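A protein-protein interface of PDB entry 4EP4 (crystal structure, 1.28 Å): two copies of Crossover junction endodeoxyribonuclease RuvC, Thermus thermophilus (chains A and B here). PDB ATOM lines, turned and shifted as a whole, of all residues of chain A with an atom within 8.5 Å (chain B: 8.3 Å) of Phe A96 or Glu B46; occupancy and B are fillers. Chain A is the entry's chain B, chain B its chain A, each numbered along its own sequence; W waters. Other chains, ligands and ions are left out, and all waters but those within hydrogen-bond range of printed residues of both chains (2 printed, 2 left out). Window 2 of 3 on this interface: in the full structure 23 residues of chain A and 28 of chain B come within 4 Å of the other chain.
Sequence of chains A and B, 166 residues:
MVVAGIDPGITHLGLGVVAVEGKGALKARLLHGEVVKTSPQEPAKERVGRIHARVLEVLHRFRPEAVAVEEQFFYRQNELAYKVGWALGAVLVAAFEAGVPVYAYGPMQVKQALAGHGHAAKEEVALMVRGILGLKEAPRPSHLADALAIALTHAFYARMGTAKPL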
ATOM      1  N   HIS A  52      11.541  23.820  -7.974  1.00  0.00           N
ATOM      2  CA  HIS A  52      12.788  24.569  -7.855  1.00  0.00           C
ATOM      3  C   HIS A  52      12.562  26.058  -8.098  1.00  0.00           C
ATOM      4  O   HIS A  52      13.040  26.905  -7.339  1.00  0.00           O
ATOM      5  CB  HIS A  52      13.830  24.045  -8.839  1.00  0.00           C
ATOM      6  CG  HIS A  52      15.034  24.927  -8.961  1.00  0.00           C
ATOM      7  ND1 HIS A  52      15.175  25.844  -9.976  1.00  0.00           N
ATOM      8  CD2 HIS A  52      16.146  25.030  -8.195  1.00  0.00           C
ATOM      9  CE1 HIS A  52      16.329  26.481  -9.833  1.00  0.00           C
ATOM     10  NE2 HIS A  52      16.936  26.003  -8.762  1.00  0.00           N
ATOM     11  N   VAL A  55      10.491  27.722  -5.153  1.00  0.00           N
ATOM     12  CA  VAL A  55      11.275  27.800  -3.925  1.00  0.00           C
ATOM     13  C   VAL A  55      12.402  28.826  -4.051  1.00  0.00           C
ATOM     14  O   VAL A  55      12.610  29.645  -3.153  1.00  0.00           O
ATOM     15  CB  VAL A  55      11.839  26.418  -3.534  1.00  0.00           C
ATOM     16  CG1 VAL A  55      12.799  26.532  -2.367  1.00  0.00           C
ATOM     17  CG2 VAL A  55      10.706  25.456  -3.207  1.00  0.00           C
ATOM     18  N   LEU A  56      13.125  28.794  -5.166  1.00  0.00           N
ATOM     19  CA  LEU A  56      14.230  29.726  -5.348  1.00  0.00           C
ATOM     20  C   LEU A  56      13.766  31.191  -5.302  1.00  0.00           C
ATOM     21  O   LEU A  56      14.408  32.029  -4.667  1.00  0.00           O
ATOM     22  CB  LEU A  56      15.003  29.425  -6.636  1.00  0.00           C
ATOM     23  CG  LEU A  56      16.201  30.350  -6.896  1.00  0.00           C
ATOM     24  CD1 LEU A  56      17.149  30.416  -5.695  1.00  0.00           C
ATOM     25  CD2 LEU A  56      16.957  29.913  -8.140  1.00  0.00           C
ATOM     26  N   LEU A  59      13.247  32.118  -1.694  1.00  0.00           N
ATOM     27  CA  LEU A  59      14.515  32.293  -0.984  1.00  0.00           C
ATOM     28  C   LEU A  59      15.188  33.622  -1.356  1.00  0.00           C
ATOM     29  O   LEU A  59      15.704  34.336  -0.496  1.00  0.00           O
ATOM     30  CB  LEU A  59      15.457  31.113  -1.226  1.00  0.00           C
ATOM     31  CG  LEU A  59      14.937  29.734  -0.824  1.00  0.00           C
ATOM     32  CD1 LEU A  59      16.039  28.692  -0.983  1.00  0.00           C
ATOM     33  CD2 LEU A  59      14.368  29.716   0.593  1.00  0.00           C
ATOM     34  N   HIS A  60      15.140  33.972  -2.632  1.00  0.00           N
ATOM     35  CA  HIS A  60      15.733  35.229  -3.093  1.00  0.00           C
ATOM     36  C   HIS A  60      14.996  36.433  -2.510  1.00  0.00           C
ATOM     37  O   HIS A  60      15.611  37.393  -2.031  1.00  0.00           O
ATOM     38  CB  HIS A  60      15.680  35.309  -4.621  1.00  0.00           C
ATOM     39  CG  HIS A  60      16.820  34.629  -5.316  1.00  0.00           C
ATOM     40  ND1 HIS A  60      16.743  34.209  -6.630  1.00  0.00           N
ATOM     41  CD2 HIS A  60      18.068  34.319  -4.897  1.00  0.00           C
ATOM     42  CE1 HIS A  60      17.895  33.670  -6.986  1.00  0.00           C
ATOM     43  NE2 HIS A  60      18.717  33.722  -5.951  1.00  0.00           N
ATOM     44  N   VAL A  67      16.102  27.425   5.797  1.00  0.00           N
ATOM     45  CA  VAL A  67      15.030  26.634   5.182  1.00  0.00           C
ATOM     46  C   VAL A  67      14.887  25.373   6.016  1.00  0.00           C
ATOM     47  O   VAL A  67      15.878  24.648   6.182  1.00  0.00           O
ATOM     48  CB  VAL A  67      15.410  26.178   3.751  1.00  0.00           C
ATOM     49  CG1 VAL A  67      14.320  25.262   3.157  1.00  0.00           C
ATOM     50  CG2 VAL A  67      15.669  27.373   2.866  1.00  0.00           C
ATOM     51  N   GLY A  89      15.482  17.400  -3.716  1.00  0.00           N
ATOM     52  CA  GLY A  89      16.609  17.745  -4.572  1.00  0.00           C
ATOM     53  C   GLY A  89      16.455  19.147  -5.142  1.00  0.00           C
ATOM     54  O   GLY A  89      17.393  19.956  -5.105  1.00  0.00           O
ATOM     55  N   ALA A  90      15.255  19.447  -5.636  1.00  0.00           N
ATOM     56  CA  ALA A  90      14.942  20.781  -6.149  1.00  0.00           C
ATOM     57  C   ALA A  90      15.099  21.843  -5.057  1.00  0.00           C
ATOM     58  O   ALA A  90      15.680  22.906  -5.294  1.00  0.00           O
ATOM     59  CB  ALA A  90      13.526  20.812  -6.732  1.00  0.00           C
ATOM     60  N   VAL A  91      14.577  21.557  -3.866  1.00  0.00           N
ATOM     61  CA  VAL A  91      14.723  22.458  -2.721  1.00  0.00           C
ATOM     62  C   VAL A  91      16.197  22.704  -2.388  1.00  0.00           C
ATOM     63  O   VAL A  91      16.615  23.843  -2.165  1.00  0.00           O
ATOM     64  CB  VAL A  91      14.001  21.902  -1.477  1.00  0.00           C
ATOM     65  CG1 VAL A  91      14.343  22.724  -0.235  1.00  0.00           C
ATOM     66  CG2 VAL A  91      12.496  21.884  -1.699  1.00  0.00           C
ATOM     67  N   LEU A  92      16.986  21.631  -2.370  1.00  0.00           N
ATOM     68  CA  LEU A  92      18.404  21.724  -2.048  1.00  0.00           C
ATOM     69  C   LEU A  92      19.192  22.516  -3.092  1.00  0.00           C
ATOM     70  O   LEU A  92      20.062  23.314  -2.737  1.00  0.00           O
ATOM     71  CB  LEU A  92      19.006  20.331  -1.848  1.00  0.00           C
ATOM     72  CG  LEU A  92      18.552  19.608  -0.577  1.00  0.00           C
ATOM     73  CD1 LEU A  92      19.084  18.179  -0.553  1.00  0.00           C
ATOM     74  CD2 LEU A  92      18.988  20.377   0.656  1.00  0.00           C
ATOM     75  N   VAL A  93      18.885  22.305  -4.369  1.00  0.00           N
ATOM     76  CA  VAL A  93      19.514  23.103  -5.423  1.00  0.00           C
ATOM     77  C   VAL A  93      19.189  24.592  -5.218  1.00  0.00           C
ATOM     78  O   VAL A  93      20.077  25.446  -5.307  1.00  0.00           O
ATOM     79  CB  VAL A  93      19.117  22.632  -6.843  1.00  0.00           C
ATOM     80  CG1 VAL A  93      19.685  23.562  -7.906  1.00  0.00           C
ATOM     81  CG2 VAL A  93      19.593  21.196  -7.087  1.00  0.00           C
ATOM     82  N   ALA A  94      17.922  24.898  -4.933  1.00  0.00           N
ATOM     83  CA  ALA A  94      17.501  26.278  -4.680  1.00  0.00           C
ATOM     84  C   ALA A  94      18.254  26.875  -3.480  1.00  0.00           C
ATOM     85  O   ALA A  94      18.758  27.998  -3.548  1.00  0.00           O
ATOM     86  CB  ALA A  94      15.999  26.351  -4.468  1.00  0.00           C
ATOM     87  N   ALA A  95      18.350  26.116  -2.387  1.00  0.00           N
ATOM     88  CA  ALA A  95      19.026  26.600  -1.188  1.00  0.00           C
ATOM     89  C   ALA A  95      20.529  26.804  -1.428  1.00  0.00           C
ATOM     90  O   ALA A  95      21.144  27.743  -0.905  1.00  0.00           O
ATOM     91  CB  ALA A  95      18.785  25.656  -0.020  1.00  0.00           C
ATOM     92  N   PHE A  96      21.110  25.913  -2.222  1.00  0.00           N
ATOM     93  CA  PHE A  96      22.498  26.030  -2.640  1.00  0.00           C
ATOM     94  C   PHE A  96      22.733  27.335  -3.404  1.00  0.00           C
ATOM     95  O   PHE A  96      23.672  28.086  -3.119  1.00  0.00           O
ATOM     96  CB  PHE A  96      22.865  24.823  -3.506  1.00  0.00           C
ATOM     97  CG  PHE A  96      24.205  24.941  -4.181  1.00  0.00           C
ATOM     98  CD1 PHE A  96      25.377  24.759  -3.462  1.00  0.00           C
ATOM     99  CD2 PHE A  96      24.287  25.219  -5.539  1.00  0.00           C
ATOM    100  CE1 PHE A  96      26.617  24.859  -4.089  1.00  0.00           C
ATOM    101  CE2 PHE A  96      25.516  25.319  -6.174  1.00  0.00           C
ATOM    102  CZ  PHE A  96      26.685  25.137  -5.445  1.00  0.00           C
ATOM    103  N   GLU A  97      21.869  27.610  -4.372  1.00  0.00           N
ATOM    104  CA  GLU A  97      22.021  28.812  -5.180  1.00  0.00           C
ATOM    105  C   GLU A  97      21.803  30.088  -4.364  1.00  0.00           C
ATOM    106  O   GLU A  97      22.545  31.064  -4.517  1.00  0.00           O
ATOM    107  CB  GLU A  97      21.085  28.767  -6.386  1.00  0.00           C
ATOM    108  CG  GLU A  97      21.322  27.560  -7.289  1.00  0.00           C
ATOM    109  CD  GLU A  97      20.610  27.682  -8.617  1.00  0.00           C
ATOM    110  OE1 GLU A  97      19.499  27.134  -8.747  1.00  0.00           O
ATOM    111  OE2 GLU A  97      21.166  28.330  -9.527  1.00  0.00           O
ATOM    112  N   ALA A  98      20.807  30.077  -3.482  1.00  0.00           N
ATOM    113  CA  ALA A  98      20.471  31.261  -2.694  1.00  0.00           C
ATOM    114  C   ALA A  98      21.362  31.443  -1.467  1.00  0.00           C
ATOM    115  O   ALA A  98      21.331  32.496  -0.827  1.00  0.00           O
ATOM    116  CB  ALA A  98      19.012  31.210  -2.288  1.00  0.00           C
ATOM    117  N   GLY A  99      22.147  30.422  -1.135  1.00  0.00           N
ATOM    118  CA  GLY A  99      23.013  30.480   0.035  1.00  0.00           C
ATOM    119  C   GLY A  99      22.234  30.560   1.345  1.00  0.00           C
ATOM    120  O   GLY A  99      22.502  31.432   2.181  1.00  0.00           O
ATOM    121  N   VAL A 100      21.271  29.652   1.515  1.00  0.00           N
ATOM    122  CA  VAL A 100      20.473  29.555   2.734  1.00  0.00           C
ATOM    123  C   VAL A 100      20.675  28.161   3.313  1.00  0.00           C
ATOM    124  O   VAL A 100      20.446  27.165   2.624  1.00  0.00           O
ATOM    125  CB  VAL A 100      18.973  29.758   2.440  1.00  0.00           C
ATOM    126  CG1 VAL A 100      18.167  29.670   3.738  1.00  0.00           C
ATOM    127  CG2 VAL A 100      18.735  31.084   1.730  1.00  0.00           C
ATOM    128  N   PRO A 101      21.095  28.077   4.583  1.00  0.00           N
ATOM    129  CA  PRO A 101      21.302  26.745   5.166  1.00  0.00           C
ATOM    130  C   PRO A 101      19.991  26.002   5.379  1.00  0.00           C
ATOM    131  O   PRO A 101      18.936  26.617   5.588  1.00  0.00           O
ATOM    132  CB  PRO A 101      21.985  27.044   6.504  1.00  0.00           C
ATOM    133  CG  PRO A 101      21.561  28.429   6.842  1.00  0.00           C
ATOM    134  CD  PRO A 101      21.465  29.153   5.519  1.00  0.00           C
ATOM    135  N   VAL A 102      20.079  24.675   5.334  1.00  0.00           N
ATOM    136  CA  VAL A 102      18.914  23.800   5.380  1.00  0.00           C
ATOM    137  C   VAL A 102      18.925  22.973   6.667  1.00  0.00           C
ATOM    138  O   VAL A 102      19.979  22.490   7.107  1.00  0.00           O
ATOM    139  CB  VAL A 102      18.898  22.851   4.152  1.00  0.00           C
ATOM    140  CG1 VAL A 102      17.632  21.976   4.141  1.00  0.00           C
ATOM    141  CG2 VAL A 102      19.019  23.643   2.874  1.00  0.00           C
ATOM    142  N   LEU A 166      20.487  19.723   8.039  1.00  0.00           N
ATOM    143  CA  LEU A 166      20.109  18.556   7.247  1.00  0.00           C
ATOM    144  C   LEU A 166      21.267  17.584   7.063  1.00  0.00           C
ATOM    145  O   LEU A 166      22.401  17.993   6.816  1.00  0.00           O
ATOM    146  CB  LEU A 166      19.573  18.981   5.883  1.00  0.00           C
ATOM    147  CG  LEU A 166      19.331  17.827   4.906  1.00  0.00           C
ATOM    148  CD1 LEU A 166      18.188  16.970   5.397  1.00  0.00           C
ATOM    149  CD2 LEU A 166      19.038  18.332   3.521  1.00  0.00           C
ATOM    150  OXT LEU A 166      21.093  16.367   7.151  1.00  0.00           O
ATOM    151  N   VAL B  36      30.877  12.569 -10.997  1.00  0.00           N
ATOM    152  CA  VAL B  36      30.764  13.710 -10.105  1.00  0.00           C
ATOM    153  C   VAL B  36      30.871  13.186  -8.684  1.00  0.00           C
ATOM    154  O   VAL B  36      30.129  12.286  -8.292  1.00  0.00           O
ATOM    155  CB  VAL B  36      29.428  14.458 -10.281  1.00  0.00           C
ATOM    156  CG1 VAL B  36      29.419  15.715  -9.427  1.00  0.00           C
ATOM    157  CG2 VAL B  36      29.210  14.809 -11.748  1.00  0.00           C
ATOM    158  N   LYS B  37      31.807  13.727  -7.916  1.00  0.00           N
ATOM    159  CA  LYS B  37      32.024  13.212  -6.574  1.00  0.00           C
ATOM    160  C   LYS B  37      31.573  14.187  -5.495  1.00  0.00           C
ATOM    161  O   LYS B  37      31.461  15.389  -5.731  1.00  0.00           O
ATOM    162  CB  LYS B  37      33.476  12.780  -6.391  1.00  0.00           C
ATOM    163  CG  LYS B  37      33.848  11.638  -7.331  1.00  0.00           C
ATOM    164  CD  LYS B  37      35.321  11.284  -7.275  1.00  0.00           C
ATOM    165  CE  LYS B  37      35.688  10.276  -8.360  1.00  0.00           C
ATOM    166  NZ  LYS B  37      35.739  10.889  -9.722  1.00  0.00           N
ATOM    167  N   THR B  38      31.287  13.639  -4.320  1.00  0.00           N
ATOM    168  CA  THR B  38      30.778  14.402  -3.195  1.00  0.00           C
ATOM    169  C   THR B  38      31.805  14.422  -2.075  1.00  0.00           C
ATOM    170  O   THR B  38      32.726  13.602  -2.044  1.00  0.00           O
ATOM    171  CB  THR B  38      29.504  13.756  -2.628  1.00  0.00           C
ATOM    172  OG1 THR B  38      29.828  12.476  -2.068  1.00  0.00           O
ATOM    173  CG2 THR B  38      28.464  13.581  -3.713  1.00  0.00           C
ATOM    174  N   SER B  39      31.632  15.351  -1.149  1.00  0.00           N
ATOM    175  CA  SER B  39      32.479  15.402   0.026  1.00  0.00           C
ATOM    176  C   SER B  39      31.634  15.240   1.283  1.00  0.00           C
ATOM    177  O   SER B  39      30.599  15.882   1.423  1.00  0.00           O
ATOM    178  CB  SER B  39      33.233  16.729   0.084  1.00  0.00           C
ATOM    179  OG  SER B  39      33.930  16.855   1.306  1.00  0.00           O
ATOM    180  N   GLN B  41      32.495  16.387   3.928  1.00  0.00           N
ATOM    181  CA  GLN B  41      32.773  17.637   4.639  1.00  0.00           C
ATOM    182  C   GLN B  41      31.956  18.834   4.159  1.00  0.00           C
ATOM    183  O   GLN B  41      32.136  19.947   4.659  1.00  0.00           O
ATOM    184  CB  GLN B  41      34.256  17.995   4.527  1.00  0.00           C
ATOM    185  CG  GLN B  41      35.188  17.016   5.184  1.00  0.00           C
ATOM    186  CD  GLN B  41      36.632  17.457   5.083  1.00  0.00           C
ATOM    187  OE1 GLN B  41      37.148  18.152   5.963  1.00  0.00           O
ATOM    188  NE2 GLN B  41      37.289  17.073   3.999  1.00  0.00           N
ATOM    189  N   GLU B  42      31.080  18.616   3.183  1.00  0.00           N
ATOM    190  CA  GLU B  42      30.222  19.689   2.692  1.00  0.00           C
ATOM    191  C   GLU B  42      28.767  19.360   2.999  1.00  0.00           C
ATOM    192  O   GLU B  42      28.407  18.183   3.123  1.00  0.00           O
ATOM    193  CB  GLU B  42      30.418  19.900   1.191  1.00  0.00           C
ATOM    194  CG  GLU B  42      29.899  18.761   0.329  1.00  0.00           C
ATOM    195  CD  GLU B  42      30.418  18.824  -1.098  1.00  0.00           C
ATOM    196  OE1 GLU B  42      31.044  19.847  -1.460  1.00  0.00           O
ATOM    197  OE2 GLU B  42      30.202  17.850  -1.855  1.00  0.00           O
ATOM    198  N   PRO B  43      27.933  20.402   3.161  1.00  0.00           N
ATOM    199  CA  PRO B  43      26.504  20.200   3.419  1.00  0.00           C
ATOM    200  C   PRO B  43      25.821  19.403   2.306  1.00  0.00           C
ATOM    201  O   PRO B  43      26.298  19.397   1.168  1.00  0.00           O
ATOM    202  CB  PRO B  43      25.955  21.630   3.439  1.00  0.00           C
ATOM    203  CG  PRO B  43      27.100  22.477   3.881  1.00  0.00           C
ATOM    204  CD  PRO B  43      28.336  21.814   3.314  1.00  0.00           C
ATOM    205  N   ALA B  44      24.699  18.764   2.632  1.00  0.00           N
ATOM    206  CA  ALA B  44      23.918  18.031   1.642  1.00  0.00           C
ATOM    207  C   ALA B  44      23.594  18.878   0.414  1.00  0.00           C
ATOM    208  O   ALA B  44      23.657  18.390  -0.713  1.00  0.00           O
ATOM    209  CB  ALA B  44      22.635  17.487   2.263  1.00  0.00           C
ATOM    210  N   LYS B  45      23.261  20.145   0.637  1.00  0.00           N
ATOM    211  CA  LYS B  45      22.868  21.026  -0.459  1.00  0.00           C
ATOM    212  C   LYS B  45      24.021  21.301  -1.426  1.00  0.00           C
ATOM    213  O   LYS B  45      23.790  21.619  -2.591  1.00  0.00           O
ATOM    214  CB  LYS B  45      22.253  22.332   0.066  1.00  0.00           C
ATOM    215  CG  LYS B  45      23.242  23.372   0.577  1.00  0.00           C
ATOM    216  CD  LYS B  45      22.500  24.621   1.055  1.00  0.00           C
ATOM    217  CE  LYS B  45      23.448  25.785   1.317  1.00  0.00           C
ATOM    218  NZ  LYS B  45      24.410  25.490   2.419  1.00  0.00           N
ATOM    219  N   GLU B  46      25.256  21.168  -0.946  1.00  0.00           N
ATOM    220  CA  GLU B  46      26.439  21.368  -1.779  1.00  0.00           C
ATOM    221  C   GLU B  46      26.623  20.195  -2.720  1.00  0.00           C
ATOM    222  O   GLU B  46      27.002  20.374  -3.871  1.00  0.00           O
ATOM    223  CB  GLU B  46      27.706  21.478  -0.930  1.00  0.00           C
ATOM    224  CG  GLU B  46      27.709  22.608   0.058  1.00  0.00           C
ATOM    225  CD  GLU B  46      27.677  23.953  -0.611  1.00  0.00           C
ATOM    226  OE1 GLU B  46      27.081  24.890  -0.038  1.00  0.00           O
ATOM    227  OE2 GLU B  46      28.264  24.075  -1.707  1.00  0.00           O
ATOM    228  N   ARG B  47      26.383  18.990  -2.216  1.00  0.00           N
ATOM    229  CA  ARG B  47      26.507  17.782  -3.025  1.00  0.00           C
ATOM    230  C   ARG B  47      25.519  17.841  -4.185  1.00  0.00           C
ATOM    231  O   ARG B  47      25.870  17.580  -5.339  1.00  0.00           O
ATOM    232  CB  ARG B  47      26.251  16.549  -2.160  1.00  0.00           C
ATOM    233  CG  ARG B  47      27.128  16.514  -0.909  1.00  0.00           C
ATOM    234  CD  ARG B  47      26.778  15.364   0.024  1.00  0.00           C
ATOM    235  NE  ARG B  47      27.565  15.427   1.255  1.00  0.00           N
ATOM    236  CZ  ARG B  47      27.114  15.083   2.458  1.00  0.00           C
ATOM    237  NH1 ARG B  47      27.906  15.179   3.517  1.00  0.00           N
ATOM    238  NH2 ARG B  47      25.873  14.641   2.608  1.00  0.00           N
ATOM    239  N   VAL B  48      24.292  18.233  -3.867  1.00  0.00           N
ATOM    240  CA  VAL B  48      23.230  18.292  -4.851  1.00  0.00           C
ATOM    241  C   VAL B  48      23.452  19.472  -5.801  1.00  0.00           C
ATOM    242  O   VAL B  48      23.242  19.356  -7.017  1.00  0.00           O
ATOM    243  CB  VAL B  48      21.862  18.351  -4.143  1.00  0.00           C
ATOM    244  CG1 VAL B  48      20.733  18.372  -5.137  1.00  0.00           C
ATOM    245  CG2 VAL B  48      21.712  17.134  -3.241  1.00  0.00           C
ATOM    246  N   GLY B  49      23.898  20.599  -5.253  1.00  0.00           N
ATOM    247  CA  GLY B  49      24.251  21.753  -6.061  1.00  0.00           C
ATOM    248  C   GLY B  49      25.347  21.469  -7.082  1.00  0.00           C
ATOM    249  O   GLY B  49      25.285  21.944  -8.217  1.00  0.00           O
ATOM    250  N   ARG B  50      26.359  20.699  -6.687  1.00  0.00           N
ATOM    251  CA  ARG B  50      27.435  20.340  -7.608  1.00  0.00           C
ATOM    252  C   ARG B  50      26.928  19.465  -8.756  1.00  0.00           C
ATOM    253  O   ARG B  50      27.341  19.628  -9.904  1.00  0.00           O
ATOM    254  CB  ARG B  50      28.557  19.601  -6.879  1.00  0.00           C
ATOM    255  CG  ARG B  50      29.605  19.036  -7.831  1.00  0.00           C
ATOM    256  CD  ARG B  50      30.754  18.358  -7.107  1.00  0.00           C
ATOM    257  NE  ARG B  50      31.409  19.259  -6.168  1.00  0.00           N
ATOM    258  CZ  ARG B  50      31.213  19.223  -4.856  1.00  0.00           C
ATOM    259  NH1 ARG B  50      31.845  20.076  -4.061  1.00  0.00           N
ATOM    260  NH2 ARG B  50      30.394  18.319  -4.335  1.00  0.00           N
ATOM    261  N   ILE B  51      26.044  18.524  -8.436  1.00  0.00           N
ATOM    262  CA  ILE B  51      25.458  17.650  -9.445  1.00  0.00           C
ATOM    263  C   ILE B  51      24.720  18.482 -10.490  1.00  0.00           C
ATOM    264  O   ILE B  51      24.918  18.303 -11.687  1.00  0.00           O
ATOM    265  CB  ILE B  51      24.498  16.623  -8.803  1.00  0.00           C
ATOM    266  CG1 ILE B  51      25.296  15.568  -8.033  1.00  0.00           C
ATOM    267  CG2 ILE B  51      23.618  15.963  -9.855  1.00  0.00           C
ATOM    268  CD1 ILE B  51      24.444  14.683  -7.149  1.00  0.00           C
ATOM    269  N   HIS B  52      23.884  19.401 -10.022  1.00  0.00           N
ATOM    270  CA  HIS B  52      23.156  20.300 -10.914  1.00  0.00           C
ATOM    271  C   HIS B  52      24.104  21.071 -11.832  1.00  0.00           C
ATOM    272  O   HIS B  52      23.893  21.120 -13.040  1.00  0.00           O
ATOM    273  CB  HIS B  52      22.299  21.262 -10.088  1.00  0.00           C
ATOM    274  CG  HIS B  52      21.656  22.346 -10.894  1.00  0.00           C
ATOM    275  ND1 HIS B  52      22.177  23.617 -10.978  1.00  0.00           N
ATOM    276  CD2 HIS B  52      20.536  22.346 -11.655  1.00  0.00           C
ATOM    277  CE1 HIS B  52      21.404  24.358 -11.750  1.00  0.00           C
ATOM    278  NE2 HIS B  52      20.398  23.611 -12.171  1.00  0.00           N
ATOM    279  N   ALA B  53      25.158  21.649 -11.259  1.00  0.00           N
ATOM    280  CA  ALA B  53      26.116  22.439 -12.030  1.00  0.00           C
ATOM    281  C   ALA B  53      26.833  21.597 -13.085  1.00  0.00           C
ATOM    282  O   ALA B  53      26.988  22.028 -14.238  1.00  0.00           O
ATOM    283  CB  ALA B  53      27.124  23.100 -11.106  1.00  0.00           C
HETATM  284  O   HOH W   1      25.145  27.646  -0.794  1.00  0.00           O
HETATM  285  O   HOH W   2      23.132  23.745   4.695  1.00  0.00           O
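Val B48 touches Gly A89 (CG1 to O, 3.7 Å). Leu A92 touches Lys B45. CG2 of Val A93 touches CG1 of Val B48, at 3.6 Å. Val A93 touches His B52 (CG1 to CG, 3.8 Å). Lys B45 touches Ala A95. Lys B45 touches Phe A96 (O to CB, 3.5 Å). Phe A96 touches Glu B46 (CE1 to OE2, 3.0 Å). Gly B49 touches Phe A96 (CA to CD2, 3.5 Å). Lys B45 touches Val A100 (CE to O, 3.6 Å). CB of Ala B44 touches CD2 of Leu A166, at 3.9 Å.
Hydrophobic or aromatic side chains of chain B that line the printed part of chain A: Ala B44, Val B48 and His B52. Hydrophobic or aromatic side chains of chain A within 4 Å of the printed part of chain B: Leu A92, Val A93, Phe A96 and Leu A166.
Water W1 lies within hydrogen-bond range of O of Phe A96 and OE1 of Glu B46. Water W2 lies within hydrogen-bond range of NZ of Lys B45 and N of Val A102.
Of the printed residues of chain B, Phe A96 touches Lys B45, Glu B46 and Gly B49. Of the printed residues of chain A, Glu B46 touches Phe A96. Gly B49 touches just one residue of chain A: Phe A96. Printed residues of chain B within 4 Å of Ala A95: Lys B45. Of the printed residues of chain B, Gly A89 touches Val B48. Printed residues of chain B within 4 Å of Val A100: Lys B45 (3.6 Å). Thr B38 touches none of the printed residues of chain A. The nearest residue of chain A that does not touch Glu B46 is Leu A92 (5.9 Å). The nearest printed residue of chain A that does not touch Val B48 is Ala A90 (5.6 Å).
Position printed for both chains: 52. Of the 11 pairs that touch across the chains among the printed residues, none has its exchanged pair printed and touching as well.
OE1 of Glu B46 is in salt-bridge range of NZ of Lys B45, 3.7 Å away. The backbone carbonyl oxygen of Ala A95 lies within hydrogen-bond range of the backbone NH of Val A100 (3.1 Å). The backbone carbonyl oxygen (O) of Val A102 sits at hydrogen-bond distance from the backbone NH (N) of Leu A166, at 3.0 Å.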
